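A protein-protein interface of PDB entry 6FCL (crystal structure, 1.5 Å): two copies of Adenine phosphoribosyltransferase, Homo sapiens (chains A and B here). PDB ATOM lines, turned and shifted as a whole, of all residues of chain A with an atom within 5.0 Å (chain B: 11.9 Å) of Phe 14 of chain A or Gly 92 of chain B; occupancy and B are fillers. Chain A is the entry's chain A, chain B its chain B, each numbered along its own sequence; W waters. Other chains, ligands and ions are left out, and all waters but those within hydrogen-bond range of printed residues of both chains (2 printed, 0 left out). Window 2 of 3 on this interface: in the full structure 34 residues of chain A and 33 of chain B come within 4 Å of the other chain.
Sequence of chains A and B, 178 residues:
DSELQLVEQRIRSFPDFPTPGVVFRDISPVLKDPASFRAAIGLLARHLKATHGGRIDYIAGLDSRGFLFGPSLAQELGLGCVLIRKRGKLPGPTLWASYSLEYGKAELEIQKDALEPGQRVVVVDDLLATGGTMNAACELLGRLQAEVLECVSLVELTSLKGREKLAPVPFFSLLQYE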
ATOM      1  N   ARG A  12      27.390  -1.420   6.137  1.00  0.00           N
ATOM      2  CA  ARG A  12      26.222  -1.463   7.009  1.00  0.00           C
ATOM      3  C   ARG A  12      25.775  -0.025   7.320  1.00  0.00           C
ATOM      4  O   ARG A  12      26.589   0.817   7.706  1.00  0.00           O
ATOM      5  CB  ARG A  12      26.602  -2.214   8.295  1.00  0.00           C
ATOM      6  CG  ARG A  12      25.442  -2.604   9.181  1.00  0.00           C
ATOM      7  CD  ARG A  12      25.894  -3.617  10.218  1.00  0.00           C
ATOM      8  NE  ARG A  12      27.223  -3.303  10.734  1.00  0.00           N
ATOM      9  CZ  ARG A  12      27.745  -3.841  11.831  1.00  0.00           C
ATOM     10  NH1 ARG A  12      28.971  -3.502  12.224  1.00  0.00           N
ATOM     11  NH2 ARG A  12      27.038  -4.705  12.544  1.00  0.00           N
ATOM     12  N   SER A  13      24.496   0.273   7.111  1.00  0.00           N
ATOM     13  CA  SER A  13      24.010   1.642   7.260  1.00  0.00           C
ATOM     14  C   SER A  13      23.130   1.803   8.493  1.00  0.00           C
ATOM     15  O   SER A  13      22.126   1.102   8.637  1.00  0.00           O
ATOM     16  CB  SER A  13      23.260   2.068   5.997  1.00  0.00           C
ATOM     17  OG  SER A  13      24.154   2.129   4.894  1.00  0.00           O
ATOM     18  N   PHE A  14      23.530   2.702   9.388  1.00  0.00           N
ATOM     19  CA  PHE A  14      22.825   2.958  10.637  1.00  0.00           C
ATOM     20  C   PHE A  14      22.144   4.323  10.637  1.00  0.00           C
ATOM     21  O   PHE A  14      22.819   5.355  10.675  1.00  0.00           O
ATOM     22  CB  PHE A  14      23.795   2.909  11.819  1.00  0.00           C
ATOM     23  CG  PHE A  14      24.321   1.536  12.131  1.00  0.00           C
ATOM     24  CD1 PHE A  14      25.475   1.074  11.524  1.00  0.00           C
ATOM     25  CD2 PHE A  14      23.708   0.748  13.096  1.00  0.00           C
ATOM     26  CE1 PHE A  14      25.983  -0.177  11.827  1.00  0.00           C
ATOM     27  CE2 PHE A  14      24.223  -0.509  13.405  1.00  0.00           C
ATOM     28  CZ  PHE A  14      25.365  -0.954  12.778  1.00  0.00           C
ATOM     29  N   PRO A  15      20.810   4.336  10.683  1.00  0.00           N
ATOM     30  CA  PRO A  15      20.093   5.615  10.724  1.00  0.00           C
ATOM     31  C   PRO A  15      20.215   6.323  12.063  1.00  0.00           C
ATOM     32  O   PRO A  15      20.375   5.679  13.105  1.00  0.00           O
ATOM     33  CB  PRO A  15      18.646   5.214  10.463  1.00  0.00           C
ATOM     34  CG  PRO A  15      18.560   3.813  10.973  1.00  0.00           C
ATOM     35  CD  PRO A  15      19.898   3.181  10.729  1.00  0.00           C
ATOM     36  N   ASP A  16      20.235   7.651  12.014  1.00  0.00           N
ATOM     37  CA  ASP A  16      20.213   8.494  13.207  1.00  0.00           C
ATOM     38  C   ASP A  16      21.427   8.358  14.120  1.00  0.00           C
ATOM     39  O   ASP A  16      21.312   8.519  15.336  1.00  0.00           O
ATOM     40  CB  ASP A  16      18.916   8.270  13.983  1.00  0.00           C
ATOM     41  CG  ASP A  16      17.690   8.395  13.100  1.00  0.00           C
ATOM     42  OD1 ASP A  16      17.624   9.361  12.304  1.00  0.00           O
ATOM     43  OD2 ASP A  16      16.794   7.525  13.181  1.00  0.00           O
ATOM     44  N   PHE A  17      22.582   8.082  13.530  1.00  0.00           N
ATOM     45  CA  PHE A  17      23.848   8.089  14.265  1.00  0.00           C
ATOM     46  C   PHE A  17      24.832   8.958  13.496  1.00  0.00           C
ATOM     47  O   PHE A  17      25.046   8.724  12.318  1.00  0.00           O
ATOM     48  CB  PHE A  17      24.430   6.684  14.419  1.00  0.00           C
ATOM     49  CG  PHE A  17      25.717   6.657  15.203  1.00  0.00           C
ATOM     50  CD1 PHE A  17      25.692   6.587  16.590  1.00  0.00           C
ATOM     51  CD2 PHE A  17      26.943   6.755  14.562  1.00  0.00           C
ATOM     52  CE1 PHE A  17      26.873   6.606  17.316  1.00  0.00           C
ATOM     53  CE2 PHE A  17      28.125   6.782  15.284  1.00  0.00           C
ATOM     54  CZ  PHE A  17      28.086   6.702  16.668  1.00  0.00           C
ATOM     55  N   VAL A  22      20.968  11.740  10.223  1.00  0.00           N
ATOM     56  CA  VAL A  22      22.242  11.276   9.638  1.00  0.00           C
ATOM     57  C   VAL A  22      22.216   9.759   9.465  1.00  0.00           C
ATOM     58  O   VAL A  22      21.799   9.036  10.380  1.00  0.00           O
ATOM     59  CB  VAL A  22      23.432  11.589  10.576  1.00  0.00           C
ATOM     60  CG1 VAL A  22      24.742  11.087   9.984  1.00  0.00           C
ATOM     61  CG2 VAL A  22      23.516  13.080  10.872  1.00  0.00           C
ATOM     62  N   VAL A  23      22.672   9.275   8.310  1.00  0.00           N
ATOM     63  CA  VAL A  23      22.860   7.843   8.103  1.00  0.00           C
ATOM     64  C   VAL A  23      24.350   7.521   8.146  1.00  0.00           C
ATOM     65  O   VAL A  23      25.139   7.986   7.310  1.00  0.00           O
ATOM     66  CB  VAL A  23      22.244   7.349   6.785  1.00  0.00           C
ATOM     67  CG1 VAL A  23      22.456   5.852   6.646  1.00  0.00           C
ATOM     68  CG2 VAL A  23      20.757   7.680   6.746  1.00  0.00           C
ATOM     69  N   PHE A  24      24.746   6.741   9.145  1.00  0.00           N
ATOM     70  CA  PHE A  24      26.143   6.370   9.297  1.00  0.00           C
ATOM     71  C   PHE A  24      26.475   5.177   8.417  1.00  0.00           C
ATOM     72  O   PHE A  24      25.802   4.154   8.455  1.00  0.00           O
ATOM     73  CB  PHE A  24      26.468   6.048  10.769  1.00  0.00           C
ATOM     74  CG  PHE A  24      27.939   5.901  11.048  1.00  0.00           C
ATOM     75  CD1 PHE A  24      28.571   4.686  10.862  1.00  0.00           C
ATOM     76  CD2 PHE A  24      28.684   6.974  11.511  1.00  0.00           C
ATOM     77  CE1 PHE A  24      29.923   4.543  11.105  1.00  0.00           C
ATOM     78  CE2 PHE A  24      30.043   6.837  11.762  1.00  0.00           C
ATOM     79  CZ  PHE A  24      30.661   5.621  11.551  1.00  0.00           C
ATOM     80  N   ASP A  26      28.921   2.311   7.871  1.00  0.00           N
ATOM     81  CA  ASP A  26      29.922   1.548   8.639  1.00  0.00           C
ATOM     82  C   ASP A  26      30.666   0.570   7.738  1.00  0.00           C
ATOM     83  O   ASP A  26      30.046  -0.333   7.178  1.00  0.00           O
ATOM     84  CB  ASP A  26      29.202   0.773   9.746  1.00  0.00           C
ATOM     85  CG  ASP A  26      30.154   0.002  10.660  1.00  0.00           C
ATOM     86  OD1 ASP A  26      31.377   0.242  10.605  1.00  0.00           O
ATOM     87  OD2 ASP A  26      29.634  -0.849  11.411  1.00  0.00           O
ATOM     88  N   LEU B  83      37.588  -4.202  14.887  1.00  0.00           N
ATOM     89  CA  LEU B  83      38.072  -2.920  15.358  1.00  0.00           C
ATOM     90  C   LEU B  83      37.678  -2.656  16.794  1.00  0.00           C
ATOM     91  O   LEU B  83      36.529  -2.871  17.175  1.00  0.00           O
ATOM     92  CB  LEU B  83      37.473  -1.781  14.533  1.00  0.00           C
ATOM     93  CG  LEU B  83      37.518  -1.897  13.013  1.00  0.00           C
ATOM     94  CD1 LEU B  83      36.876  -0.667  12.393  1.00  0.00           C
ATOM     95  CD2 LEU B  83      38.958  -2.070  12.576  1.00  0.00           C
ATOM     96  N   ARG B  85      37.745   0.716  19.120  1.00  0.00           N
ATOM     97  CA  ARG B  85      37.890   2.147  18.894  1.00  0.00           C
ATOM     98  C   ARG B  85      37.826   3.003  20.135  1.00  0.00           C
ATOM     99  O   ARG B  85      37.331   2.581  21.173  1.00  0.00           O
ATOM    100  CB  ARG B  85      36.795   2.624  17.947  1.00  0.00           C
ATOM    101  CG  ARG B  85      36.836   1.979  16.579  1.00  0.00           C
ATOM    102  CD  ARG B  85      36.583   3.029  15.515  1.00  0.00           C
ATOM    103  NE  ARG B  85      37.548   4.118  15.636  1.00  0.00           N
ATOM    104  CZ  ARG B  85      37.512   5.241  14.925  1.00  0.00           C
ATOM    105  NH1 ARG B  85      36.559   5.431  14.026  1.00  0.00           N
ATOM    106  NH2 ARG B  85      38.427   6.179  15.124  1.00  0.00           N
ATOM    107  N   LYS B  86      38.302   4.241  20.022  1.00  0.00           N
ATOM    108  CA  LYS B  86      38.071   5.207  21.081  1.00  0.00           C
ATOM    109  C   LYS B  86      36.568   5.409  21.185  1.00  0.00           C
ATOM    110  O   LYS B  86      35.854   5.375  20.181  1.00  0.00           O
ATOM    111  CB  LYS B  86      38.777   6.534  20.785  1.00  0.00           C
ATOM    112  CG  LYS B  86      40.273   6.359  20.594  1.00  0.00           C
ATOM    113  CD  LYS B  86      41.072   7.480  21.234  1.00  0.00           C
ATOM    114  CE  LYS B  86      42.556   7.318  20.944  1.00  0.00           C
ATOM    115  NZ  LYS B  86      43.010   5.913  21.145  1.00  0.00           N
ATOM    116  N   ARG B  87      36.075   5.572  22.405  1.00  0.00           N
ATOM    117  CA  ARG B  87      34.641   5.677  22.618  1.00  0.00           C
ATOM    118  C   ARG B  87      33.989   6.852  21.888  1.00  0.00           C
ATOM    119  O   ARG B  87      34.572   7.934  21.795  1.00  0.00           O
ATOM    120  CB  ARG B  87      34.336   5.773  24.109  1.00  0.00           C
ATOM    121  CG  ARG B  87      32.846   5.843  24.382  1.00  0.00           C
ATOM    122  CD  ARG B  87      32.520   5.717  25.849  1.00  0.00           C
ATOM    123  NE  ARG B  87      31.083   5.854  26.055  1.00  0.00           N
ATOM    124  CZ  ARG B  87      30.535   6.194  27.214  1.00  0.00           C
ATOM    125  NH1 ARG B  87      29.216   6.338  27.322  1.00  0.00           N
ATOM    126  NH2 ARG B  87      31.321   6.421  28.252  1.00  0.00           N
ATOM    127  N   GLY B  88      32.804   6.603  21.328  1.00  0.00           N
ATOM    128  CA  GLY B  88      32.018   7.641  20.644  1.00  0.00           C
ATOM    129  C   GLY B  88      32.046   7.537  19.132  1.00  0.00           C
ATOM    130  O   GLY B  88      31.333   8.270  18.450  1.00  0.00           O
ATOM    131  N   LYS B  89      32.810   6.581  18.605  1.00  0.00           N
ATOM    132  CA  LYS B  89      33.043   6.490  17.164  1.00  0.00           C
ATOM    133  C   LYS B  89      32.236   5.410  16.437  1.00  0.00           C
ATOM    134  O   LYS B  89      32.068   5.467  15.210  1.00  0.00           O
ATOM    135  CB  LYS B  89      34.530   6.237  16.911  1.00  0.00           C
ATOM    136  CG  LYS B  89      35.438   7.360  17.395  1.00  0.00           C
ATOM    137  CD  LYS B  89      35.217   8.628  16.591  1.00  0.00           C
ATOM    138  CE  LYS B  89      35.859   9.835  17.257  1.00  0.00           C
ATOM    139  NZ  LYS B  89      37.294   9.599  17.575  1.00  0.00           N
ATOM    140  N   LEU B  90      31.789   4.400  17.171  1.00  0.00           N
ATOM    141  CA  LEU B  90      31.101   3.259  16.575  1.00  0.00           C
ATOM    142  C   LEU B  90      29.585   3.362  16.686  1.00  0.00           C
ATOM    143  O   LEU B  90      29.064   3.701  17.742  1.00  0.00           O
ATOM    144  CB  LEU B  90      31.560   1.967  17.262  1.00  0.00           C
ATOM    145  CG  LEU B  90      33.003   1.506  17.011  1.00  0.00           C
ATOM    146  CD1 LEU B  90      33.386   0.376  17.946  1.00  0.00           C
ATOM    147  CD2 LEU B  90      33.197   1.068  15.567  1.00  0.00           C
ATOM    148  N   PRO B  91      28.866   3.001  15.607  1.00  0.00           N
ATOM    149  CA  PRO B  91      27.416   2.929  15.622  1.00  0.00           C
ATOM    150  C   PRO B  91      26.927   1.617  16.239  1.00  0.00           C
ATOM    151  O   PRO B  91      27.709   0.661  16.366  1.00  0.00           O
ATOM    152  CB  PRO B  91      27.062   2.954  14.132  1.00  0.00           C
ATOM    153  CG  PRO B  91      28.193   2.235  13.493  1.00  0.00           C
ATOM    154  CD  PRO B  91      29.418   2.570  14.309  1.00  0.00           C
ATOM    155  N   GLY B  92      25.650   1.574  16.601  1.00  0.00           N
ATOM    156  CA  GLY B  92      25.040   0.366  17.158  1.00  0.00           C
ATOM    157  C   GLY B  92      25.391   0.170  18.628  1.00  0.00           C
ATOM    158  O   GLY B  92      26.132   0.957  19.209  1.00  0.00           O
ATOM    159  N   PRO B  93      24.867  -0.894  19.234  1.00  0.00           N
ATOM    160  CA  PRO B  93      25.114  -1.151  20.660  1.00  0.00           C
ATOM    161  C   PRO B  93      26.573  -1.473  20.941  1.00  0.00           C
ATOM    162  O   PRO B  93      27.188  -2.208  20.181  1.00  0.00           O
ATOM    163  CB  PRO B  93      24.242  -2.376  20.955  1.00  0.00           C
ATOM    164  CG  PRO B  93      23.174  -2.330  19.923  1.00  0.00           C
ATOM    165  CD  PRO B  93      23.806  -1.756  18.690  1.00  0.00           C
ATOM    166  N   THR B  94      27.132  -0.861  21.978  1.00  0.00           N
ATOM    167  CA  THR B  94      28.543  -1.034  22.275  1.00  0.00           C
ATOM    168  C   THR B  94      28.767  -1.325  23.743  1.00  0.00           C
ATOM    169  O   THR B  94      27.875  -1.148  24.575  1.00  0.00           O
ATOM    170  CB  THR B  94      29.347   0.242  21.997  1.00  0.00           C
ATOM    171  OG1 THR B  94      28.839   1.302  22.815  1.00  0.00           O
ATOM    172  CG2 THR B  94      29.302   0.638  20.510  1.00  0.00           C
ATOM    173  N   LEU B  95      29.970  -1.812  24.025  1.00  0.00           N
ATOM    174  CA  LEU B  95      30.509  -1.946  25.375  1.00  0.00           C
ATOM    175  C   LEU B  95      31.752  -1.058  25.402  1.00  0.00           C
ATOM    176  O   LEU B  95      32.403  -0.882  24.360  1.00  0.00           O
ATOM    177  CB  LEU B  95      30.932  -3.400  25.649  1.00  0.00           C
ATOM    178  CG  LEU B  95      29.937  -4.532  25.389  1.00  0.00           C
ATOM    179  CD1 LEU B  95      30.592  -5.890  25.608  1.00  0.00           C
ATOM    180  CD2 LEU B  95      28.727  -4.374  26.291  1.00  0.00           C
ATOM    181  N   TRP B  96      32.104  -0.516  26.570  1.00  0.00           N
ATOM    182  CA  TRP B  96      33.311   0.283  26.696  1.00  0.00           C
ATOM    183  C   TRP B  96      34.077   0.002  27.990  1.00  0.00           C
ATOM    184  O   TRP B  96      33.524  -0.524  28.960  1.00  0.00           O
ATOM    185  CB  TRP B  96      33.008   1.780  26.558  1.00  0.00           C
ATOM    186  CG  TRP B  96      32.064   2.323  27.561  1.00  0.00           C
ATOM    187  CD1 TRP B  96      32.366   2.790  28.812  1.00  0.00           C
ATOM    188  CD2 TRP B  96      30.661   2.487  27.398  1.00  0.00           C
ATOM    189  NE1 TRP B  96      31.222   3.211  29.444  1.00  0.00           N
ATOM    190  CE2 TRP B  96      30.163   3.052  28.591  1.00  0.00           C
ATOM    191  CE3 TRP B  96      29.770   2.227  26.352  1.00  0.00           C
ATOM    192  CZ2 TRP B  96      28.819   3.354  28.765  1.00  0.00           C
ATOM    193  CZ3 TRP B  96      28.437   2.527  26.529  1.00  0.00           C
ATOM    194  CH2 TRP B  96      27.975   3.096  27.722  1.00  0.00           C
ATOM    195  N   LEU B 108      38.005   2.855  25.597  1.00  0.00           N
ATOM    196  CA  LEU B 108      37.880   2.095  24.357  1.00  0.00           C
ATOM    197  C   LEU B 108      36.482   1.467  24.265  1.00  0.00           C
ATOM    198  O   LEU B 108      35.801   1.282  25.266  1.00  0.00           O
ATOM    199  CB  LEU B 108      38.927   0.988  24.293  1.00  0.00           C
ATOM    200  CG  LEU B 108      40.393   1.408  24.150  1.00  0.00           C
ATOM    201  CD1 LEU B 108      41.238   0.166  23.914  1.00  0.00           C
ATOM    202  CD2 LEU B 108      40.590   2.406  23.022  1.00  0.00           C
ATOM    203  N   GLU B 109      36.094   1.085  23.057  1.00  0.00           N
ATOM    204  CA  GLU B 109      34.756   0.560  22.825  1.00  0.00           C
ATOM    205  C   GLU B 109      34.765  -0.462  21.700  1.00  0.00           C
ATOM    206  O   GLU B 109      35.654  -0.463  20.835  1.00  0.00           O
ATOM    207  CB  GLU B 109      33.807   1.704  22.444  1.00  0.00           C
ATOM    208  CG  GLU B 109      34.264   2.424  21.189  1.00  0.00           C
ATOM    209  CD  GLU B 109      33.204   3.314  20.561  1.00  0.00           C
ATOM    210  OE1 GLU B 109      32.141   3.541  21.186  1.00  0.00           O
ATOM    211  OE2 GLU B 109      33.470   3.809  19.440  1.00  0.00           O
ATOM    212  N   ILE B 110      33.786  -1.350  21.728  1.00  0.00           N
ATOM    213  CA  ILE B 110      33.639  -2.382  20.720  1.00  0.00           C
ATOM    214  C   ILE B 110      32.151  -2.614  20.513  1.00  0.00           C
ATOM    215  O   ILE B 110      31.360  -2.438  21.444  1.00  0.00           O
ATOM    216  CB  ILE B 110      34.327  -3.698  21.154  1.00  0.00           C
ATOM    217  CG1 ILE B 110      34.504  -4.648  19.974  1.00  0.00           C
ATOM    218  CG2 ILE B 110      33.551  -4.378  22.259  1.00  0.00           C
ATOM    219  CD1 ILE B 110      35.462  -5.791  20.275  1.00  0.00           C
ATOM    220  N   GLN B 111      31.755  -2.932  19.277  1.00  0.00           N
ATOM    221  CA  GLN B 111      30.358  -3.273  18.999  1.00  0.00           C
ATOM    222  C   GLN B 111      30.018  -4.597  19.686  1.00  0.00           C
ATOM    223  O   GLN B 111      30.845  -5.518  19.713  1.00  0.00           O
ATOM    224  CB  GLN B 111      30.119  -3.343  17.487  1.00  0.00           C
ATOM    225  CG  GLN B 111      30.141  -1.964  16.821  1.00  0.00           C
ATOM    226  CD  GLN B 111      30.114  -1.990  15.291  1.00  0.00           C
ATOM    227  OE1 GLN B 111      30.697  -2.869  14.647  1.00  0.00           O
ATOM    228  NE2 GLN B 111      29.483  -0.973  14.700  1.00  0.00           N
ATOM    229  N   LYS B 112      28.842  -4.656  20.308  1.00  0.00           N
ATOM    230  CA  LYS B 112      28.393  -5.870  21.000  1.00  0.00           C
ATOM    231  C   LYS B 112      28.360  -7.066  20.054  1.00  0.00           C
ATOM    232  O   LYS B 112      28.428  -8.200  20.514  1.00  0.00           O
ATOM    233  CB  LYS B 112      27.004  -5.689  21.624  1.00  0.00           C
ATOM    234  CG  LYS B 112      26.917  -4.676  22.754  1.00  0.00           C
ATOM    235  CD  LYS B 112      25.641  -4.883  23.559  1.00  0.00           C
ATOM    236  CE  LYS B 112      25.379  -3.746  24.536  1.00  0.00           C
ATOM    237  NZ  LYS B 112      24.125  -3.976  25.318  1.00  0.00           N
ATOM    238  N   ASP B 113      28.223  -6.826  18.750  1.00  0.00           N
ATOM    239  CA  ASP B 113      28.175  -7.931  17.788  1.00  0.00           C
ATOM    240  C   ASP B 113      29.483  -8.152  17.017  1.00  0.00           C
ATOM    241  O   ASP B 113      29.505  -8.840  15.996  1.00  0.00           O
ATOM    242  CB  ASP B 113      26.990  -7.768  16.821  1.00  0.00           C
ATOM    243  CG  ASP B 113      27.150  -6.589  15.879  1.00  0.00           C
ATOM    244  OD1 ASP B 113      28.130  -5.834  16.022  1.00  0.00           O
ATOM    245  OD2 ASP B 113      26.289  -6.425  14.986  1.00  0.00           O
ATOM    246  N   ALA B 114      30.595  -7.647  17.540  1.00  0.00           N
ATOM    247  CA  ALA B 114      31.868  -7.775  16.839  1.00  0.00           C
ATOM    248  C   ALA B 114      32.372  -9.221  16.771  1.00  0.00           C
ATOM    249  O   ALA B 114      33.002  -9.626  15.792  1.00  0.00           O
ATOM    250  CB  ALA B 114      32.914  -6.879  17.490  1.00  0.00           C
ATOM    251  N   LEU B 144      32.734 -10.139  25.539  1.00  0.00           N
ATOM    252  CA  LEU B 144      32.020 -10.744  24.418  1.00  0.00           C
ATOM    253  C   LEU B 144      32.203 -12.267  24.446  1.00  0.00           C
ATOM    254  O   LEU B 144      31.760 -12.970  23.542  1.00  0.00           O
ATOM    255  CB  LEU B 144      32.523 -10.187  23.085  1.00  0.00           C
ATOM    256  CG  LEU B 144      32.228  -8.712  22.811  1.00  0.00           C
ATOM    257  CD1 LEU B 144      32.740  -8.344  21.427  1.00  0.00           C
ATOM    258  CD2 LEU B 144      30.754  -8.383  22.947  1.00  0.00           C
HETATM  259  O   HOH W   1      26.252  -3.380  15.685  1.00  0.00           O
HETATM  260  O   HOH W   2      30.133  -5.495  14.509  1.00  0.00           O
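The side-chain amide nitrogen of Gln 111 of chain B is in hydrogen-bond range of the side-chain carboxylate of Asp 26 of chain A.
The guanidinium group (NH1) of Arg 12 of chain A is in hydrogen-bond range of the side-chain amide oxygen (OE1) of Gln 111 of chain B, at 3.0 Å.
The guanidinium group (NH2) of Arg 12 of chain A lies within salt-bridge range of the side-chain carboxylate (OD2) of Asp 113 of chain B (3.1 Å).
The side-chain carboxylate (OE2) of Glu 109 of chain B is in hydrogen-bond range of the backbone NH (N) of Leu 90 of chain B (2.9 Å).
The side-chain carboxylate of Glu 109 of chain B is in hydrogen-bond range of the backbone NH of Lys 89 of chain B, 3.0 Å away.
The side-chain carboxylate (OD2) of Asp 26 of chain A lies within salt-bridge range of the guanidinium group (NH1) of Arg 12 of chain A (2.9 Å).
The backbone carbonyl oxygen of Pro 91 of chain B is in hydrogen-bond range of the side-chain amide nitrogen of Gln 111 of chain B (2.9 Å).
The backbone carbonyl oxygen of Val 22 of chain A sits at hydrogen-bond distance from the backbone NH of Phe 17 of chain A, 3.4 Å away.
The backbone carbonyl oxygen (O) of Phe 14 of chain A sits at hydrogen-bond distance from the backbone NH (N) of Phe 24 of chain A (2.8 Å).
CD1 of Phe 14 of chain A touches CG of Pro 91 of chain B, 3.6 Å away.
Phe 14 of chain A touches Gly 92 of chain B (CE2 to CA, 3.9 Å).
O of Leu 90 of chain B touches CZ of Phe 17 of chain A (3.3 Å).
CB of Pro 91 of chain B touches CD2 of Phe 17 of chain A, at 3.8 Å.
CZ of Phe 24 of chain A touches O of Lys 89 of chain B, 3.9 Å away.
Phe 24 of chain A touches Pro 91 of chain B.
Asp 26 of chain A touches Pro 91 of chain B.
No residue of chain B comes within 4 Å of Ser 13 of chain A.
No residue of chain B comes within 4 Å of Pro 15 of chain A.
No residue of chain B comes within 4 Å of Asp 16 of chain A.
Of chain B, only Leu 90 and Pro 91 come within 4 Å of Phe 17 of chain A.
Phe 24 of chain A touches just these residues of chain B: Lys 89 and Pro 91.
Printed residues of chain B within 4 Å of Asp 26 of chain A: Pro 91 (3.99 Å) and Gln 111 (3.3 Å).
Printed residues of chain A within 4 Å of Lys 89 of chain B: Phe 24 (3.9 Å).
Of the printed residues of chain A, Leu 90 of chain B touches Phe 17 (3.3 Å).
Gly 92 of chain B touches just one residue of chain A: Phe 14 (3.9 Å).
Glu 109 of chain B touches none of the printed residues of chain A.
Of the 10 printed residues of chain A, 5 touch a printed residue of chain B.
Of the 21 printed residues of chain B, 6 touch a printed residue of chain A.
Hydrophobic or aromatic side chains of chain B within 4 Å of the printed part of chain A: Pro 91.
Among the printed residues, 10 pairs touch across the chains.
Among the printed residues, Asp or Glu carboxylates within 4 Å of a Lys or Arg side-chain nitrogen of the other chain: Arg 12 of chain A with Asp 113 of chain B (3.1 Å).
No position is printed for both chains.
Water W2 lies within hydrogen-bond range of the side-chain carboxylate (OD1) of Asp 113 of chain B, the side-chain amide oxygen (OE1) of Gln 111 of chain B and the guanidinium group (NH1) of Arg 12 of chain A.
Water W1 bridges OD1 of Asp 113 of chain B (3.1 Å) and NH2 of Arg 12 of chain A (3.5 Å).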
